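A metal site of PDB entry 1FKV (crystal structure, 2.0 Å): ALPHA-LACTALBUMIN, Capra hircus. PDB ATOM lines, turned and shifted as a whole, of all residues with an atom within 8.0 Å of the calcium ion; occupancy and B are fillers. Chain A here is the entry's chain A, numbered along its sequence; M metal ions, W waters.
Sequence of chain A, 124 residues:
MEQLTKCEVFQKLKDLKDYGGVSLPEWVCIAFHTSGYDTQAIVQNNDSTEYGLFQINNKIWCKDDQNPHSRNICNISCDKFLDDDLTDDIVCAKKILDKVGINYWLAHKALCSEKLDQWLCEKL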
ATOM      1  N   THR A  39     -17.065  14.305 -10.563  1.00  0.00           N
ATOM      2  CA  THR A  39     -18.357  14.423 -11.231  1.00  0.00           C
ATOM      3  C   THR A  39     -19.360  15.283 -10.443  1.00  0.00           C
ATOM      4  O   THR A  39     -20.444  15.586 -10.948  1.00  0.00           O
ATOM      5  CB  THR A  39     -18.977  13.033 -11.495  1.00  0.00           C
ATOM      6  OG1 THR A  39     -19.078  12.297 -10.273  1.00  0.00           O
ATOM      7  CG2 THR A  39     -18.124  12.237 -12.468  1.00  0.00           C
ATOM      8  N   ILE A  76     -32.044  21.384 -19.758  1.00  0.00           N
ATOM      9  CA  ILE A  76     -31.957  20.508 -18.605  1.00  0.00           C
ATOM     10  C   ILE A  76     -31.590  21.295 -17.367  1.00  0.00           C
ATOM     11  O   ILE A  76     -31.064  22.407 -17.466  1.00  0.00           O
ATOM     12  CB  ILE A  76     -30.897  19.417 -18.869  1.00  0.00           C
ATOM     13  CG1 ILE A  76     -30.934  18.338 -17.789  1.00  0.00           C
ATOM     14  CG2 ILE A  76     -29.531  20.054 -18.972  1.00  0.00           C
ATOM     15  CD1 ILE A  76     -29.951  17.225 -18.041  1.00  0.00           C
ATOM     16  N   SER A  77     -31.871  20.719 -16.198  1.00  0.00           N
ATOM     17  CA  SER A  77     -31.513  21.359 -14.936  1.00  0.00           C
ATOM     18  C   SER A  77     -30.055  20.981 -14.655  1.00  0.00           C
ATOM     19  O   SER A  77     -29.671  19.821 -14.816  1.00  0.00           O
ATOM     20  CB  SER A  77     -32.415  20.880 -13.816  1.00  0.00           C
ATOM     21  OG  SER A  77     -32.511  19.471 -13.810  1.00  0.00           O
ATOM     22  N   CYS A  78     -29.266  21.972 -14.251  1.00  0.00           N
ATOM     23  CA  CYS A  78     -27.843  21.771 -13.968  1.00  0.00           C
ATOM     24  C   CYS A  78     -27.515  20.685 -12.959  1.00  0.00           C
ATOM     25  O   CYS A  78     -26.466  20.055 -13.045  1.00  0.00           O
ATOM     26  CB  CYS A  78     -27.241  23.080 -13.481  1.00  0.00           C
ATOM     27  SG  CYS A  78     -27.454  24.481 -14.628  1.00  0.00           S
ATOM     28  N   ASP A  79     -28.407  20.458 -12.009  1.00  0.00           N
ATOM     29  CA  ASP A  79     -28.183  19.441 -10.980  1.00  0.00           C
ATOM     30  C   ASP A  79     -28.057  18.064 -11.596  1.00  0.00           C
ATOM     31  O   ASP A  79     -27.593  17.129 -10.949  1.00  0.00           O
ATOM     32  CB  ASP A  79     -29.321  19.461  -9.958  1.00  0.00           C
ATOM     33  CG  ASP A  79     -30.666  19.170 -10.590  1.00  0.00           C
ATOM     34  OD1 ASP A  79     -31.210  18.064 -10.370  1.00  0.00           O
ATOM     35  OD2 ASP A  79     -31.167  20.050 -11.322  1.00  0.00           O
ATOM     36  N   LYS A  80     -28.476  17.943 -12.854  1.00  0.00           N
ATOM     37  CA  LYS A  80     -28.392  16.665 -13.540  1.00  0.00           C
ATOM     38  C   LYS A  80     -26.937  16.307 -13.805  1.00  0.00           C
ATOM     39  O   LYS A  80     -26.601  15.139 -13.944  1.00  0.00           O
ATOM     40  CB  LYS A  80     -29.168  16.724 -14.851  1.00  0.00           C
ATOM     41  CG  LYS A  80     -30.462  15.914 -14.852  1.00  0.00           C
ATOM     42  CD  LYS A  80     -31.320  16.243 -13.650  1.00  0.00           C
ATOM     43  CE  LYS A  80     -32.769  16.489 -14.051  1.00  0.00           C
ATOM     44  NZ  LYS A  80     -33.518  17.244 -12.996  1.00  0.00           N
ATOM     45  N   PHE A  81     -26.076  17.320 -13.871  1.00  0.00           N
ATOM     46  CA  PHE A  81     -24.654  17.102 -14.131  1.00  0.00           C
ATOM     47  C   PHE A  81     -23.848  16.845 -12.852  1.00  0.00           C
ATOM     48  O   PHE A  81     -22.619  16.946 -12.860  1.00  0.00           O
ATOM     49  CB  PHE A  81     -24.050  18.303 -14.861  1.00  0.00           C
ATOM     50  CG  PHE A  81     -24.750  18.641 -16.151  1.00  0.00           C
ATOM     51  CD1 PHE A  81     -24.971  19.968 -16.506  1.00  0.00           C
ATOM     52  CD2 PHE A  81     -25.156  17.627 -17.027  1.00  0.00           C
ATOM     53  CE1 PHE A  81     -25.600  20.290 -17.708  1.00  0.00           C
ATOM     54  CE2 PHE A  81     -25.780  17.936 -18.228  1.00  0.00           C
ATOM     55  CZ  PHE A  81     -25.999  19.280 -18.577  1.00  0.00           C
ATOM     56  N   LEU A  82     -24.532  16.503 -11.764  1.00  0.00           N
ATOM     57  CA  LEU A  82     -23.852  16.254 -10.499  1.00  0.00           C
ATOM     58  C   LEU A  82     -24.052  14.829  -9.994  1.00  0.00           C
ATOM     59  O   LEU A  82     -23.677  14.510  -8.872  1.00  0.00           O
ATOM     60  CB  LEU A  82     -24.335  17.232  -9.432  1.00  0.00           C
ATOM     61  CG  LEU A  82     -24.057  18.706  -9.711  1.00  0.00           C
ATOM     62  CD1 LEU A  82     -24.608  19.543  -8.565  1.00  0.00           C
ATOM     63  CD2 LEU A  82     -22.565  18.928  -9.860  1.00  0.00           C
ATOM     64  N   ASP A  83     -24.653  13.980 -10.820  1.00  0.00           N
ATOM     65  CA  ASP A  83     -24.867  12.599 -10.413  1.00  0.00           C
ATOM     66  C   ASP A  83     -23.886  11.679 -11.120  1.00  0.00           C
ATOM     67  O   ASP A  83     -23.032  12.127 -11.876  1.00  0.00           O
ATOM     68  CB  ASP A  83     -26.321  12.153 -10.679  1.00  0.00           C
ATOM     69  CG  ASP A  83     -26.737  12.327 -12.122  1.00  0.00           C
ATOM     70  OD1 ASP A  83     -27.919  12.661 -12.351  1.00  0.00           O
ATOM     71  OD2 ASP A  83     -25.897  12.126 -13.011  1.00  0.00           O
ATOM     72  N   ASP A  84     -24.028  10.378 -10.869  1.00  0.00           N
ATOM     73  CA  ASP A  84     -23.146   9.373 -11.434  1.00  0.00           C
ATOM     74  C   ASP A  84     -23.347   9.018 -12.892  1.00  0.00           C
ATOM     75  O   ASP A  84     -22.448   8.449 -13.519  1.00  0.00           O
ATOM     76  CB  ASP A  84     -23.222   8.098 -10.590  1.00  0.00           C
ATOM     77  CG  ASP A  84     -22.555   8.246  -9.231  1.00  0.00           C
ATOM     78  OD1 ASP A  84     -23.104   7.717  -8.241  1.00  0.00           O
ATOM     79  OD2 ASP A  84     -21.487   8.904  -9.170  1.00  0.00           O
ATOM     80  N   ASP A  85     -24.507   9.339 -13.451  1.00  0.00           N
ATOM     81  CA  ASP A  85     -24.780   9.008 -14.851  1.00  0.00           C
ATOM     82  C   ASP A  85     -24.299  10.078 -15.827  1.00  0.00           C
ATOM     83  O   ASP A  85     -24.944  11.111 -15.987  1.00  0.00           O
ATOM     84  CB  ASP A  85     -26.278   8.771 -15.077  1.00  0.00           C
ATOM     85  CG  ASP A  85     -26.645   8.633 -16.542  1.00  0.00           C
ATOM     86  OD1 ASP A  85     -26.112   7.714 -17.195  1.00  0.00           O
ATOM     87  OD2 ASP A  85     -27.443   9.458 -17.042  1.00  0.00           O
ATOM     88  N   LEU A  86     -23.194   9.838 -16.509  1.00  0.00           N
ATOM     89  CA  LEU A  86     -22.654  10.815 -17.436  1.00  0.00           C
ATOM     90  C   LEU A  86     -23.356  10.908 -18.778  1.00  0.00           C
ATOM     91  O   LEU A  86     -22.987  11.717 -19.629  1.00  0.00           O
ATOM     92  CB  LEU A  86     -21.167  10.562 -17.637  1.00  0.00           C
ATOM     93  CG  LEU A  86     -20.363  10.696 -16.332  1.00  0.00           C
ATOM     94  CD1 LEU A  86     -18.879  10.532 -16.620  1.00  0.00           C
ATOM     95  CD2 LEU A  86     -20.635  12.069 -15.703  1.00  0.00           C
ATOM     96  N   THR A  87     -24.387  10.105 -18.966  1.00  0.00           N
ATOM     97  CA  THR A  87     -25.138  10.096 -20.223  1.00  0.00           C
ATOM     98  C   THR A  87     -25.598  11.470 -20.664  1.00  0.00           C
ATOM     99  O   THR A  87     -25.317  11.883 -21.794  1.00  0.00           O
ATOM    100  CB  THR A  87     -26.353   9.166 -20.134  1.00  0.00           C
ATOM    101  OG1 THR A  87     -25.910   7.826 -19.873  1.00  0.00           O
ATOM    102  CG2 THR A  87     -27.130   9.180 -21.437  1.00  0.00           C
ATOM    103  N   ASP A  88     -26.311  12.210 -19.801  1.00  0.00           N
ATOM    104  CA  ASP A  88     -26.761  13.537 -20.215  1.00  0.00           C
ATOM    105  C   ASP A  88     -25.613  14.552 -20.266  1.00  0.00           C
ATOM    106  O   ASP A  88     -25.648  15.472 -21.074  1.00  0.00           O
ATOM    107  CB  ASP A  88     -27.903  14.052 -19.336  1.00  0.00           C
ATOM    108  CG  ASP A  88     -27.676  13.815 -17.856  1.00  0.00           C
ATOM    109  OD1 ASP A  88     -26.535  13.520 -17.470  1.00  0.00           O
ATOM    110  OD2 ASP A  88     -28.655  13.908 -17.088  1.00  0.00           O
ATOM    111  N   ASP A  89     -24.613  14.378 -19.400  1.00  0.00           N
ATOM    112  CA  ASP A  89     -23.451  15.289 -19.396  1.00  0.00           C
ATOM    113  C   ASP A  89     -22.791  15.213 -20.770  1.00  0.00           C
ATOM    114  O   ASP A  89     -22.383  16.232 -21.333  1.00  0.00           O
ATOM    115  CB  ASP A  89     -22.413  14.843 -18.369  1.00  0.00           C
ATOM    116  CG  ASP A  89     -22.917  14.948 -16.955  1.00  0.00           C
ATOM    117  OD1 ASP A  89     -22.303  15.692 -16.162  1.00  0.00           O
ATOM    118  OD2 ASP A  89     -23.922  14.289 -16.644  1.00  0.00           O
ATOM    119  N   ILE A  90     -22.680  14.003 -21.292  1.00  0.00           N
ATOM    120  CA  ILE A  90     -22.073  13.776 -22.596  1.00  0.00           C
ATOM    121  C   ILE A  90     -22.900  14.379 -23.732  1.00  0.00           C
ATOM    122  O   ILE A  90     -22.353  14.967 -24.661  1.00  0.00           O
ATOM    123  CB  ILE A  90     -21.869  12.260 -22.830  1.00  0.00           C
ATOM    124  CG1 ILE A  90     -20.673  11.769 -22.011  1.00  0.00           C
ATOM    125  CG2 ILE A  90     -21.634  11.980 -24.294  1.00  0.00           C
ATOM    126  CD1 ILE A  90     -20.690  10.288 -21.702  1.00  0.00           C
HETATM  127 CA    CA M   1     -25.513  13.192 -15.218  1.00  0.00          CA
HETATM  128  O   HOH W   1     -23.361  13.637 -13.861  1.00  0.00           O
HETATM  129  O   HOH W   2     -28.141  12.223 -15.136  1.00  0.00           O
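The calcium ion is bound by the backbone carbonyl oxygen of Asp 85, the side-chain carboxylate of Asp 89, the side-chain carboxylate of Asp 83, the side-chain carboxylate of Asp 88, the backbone carbonyl oxygen of Lys 80, water W1 and water W2.
Water W1 lies within hydrogen-bond range of the backbone carbonyl oxygen (O) of Asp 83 (2.5 Å) and the side-chain carboxylate (OD1) of Asp 89 (3.3 Å).
OG1 of Thr 87 lies within hydrogen-bond range of OD1 of Asp 85 (2.7 Å).
The side-chain carboxylate (OD1) of Asp 79 is in salt-bridge range of the side-chain amino group (NZ) of Lys 80 (3.6 Å).
The side-chain amino group of Lys 80 lies within hydrogen-bond range of the side-chain hydroxyl of Ser 77 (2.6 Å).
Five residues have an atom within 4 Å of the calcium ion: Lys 80, Asp 83, Asp 85, Asp 88 and Asp 89.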
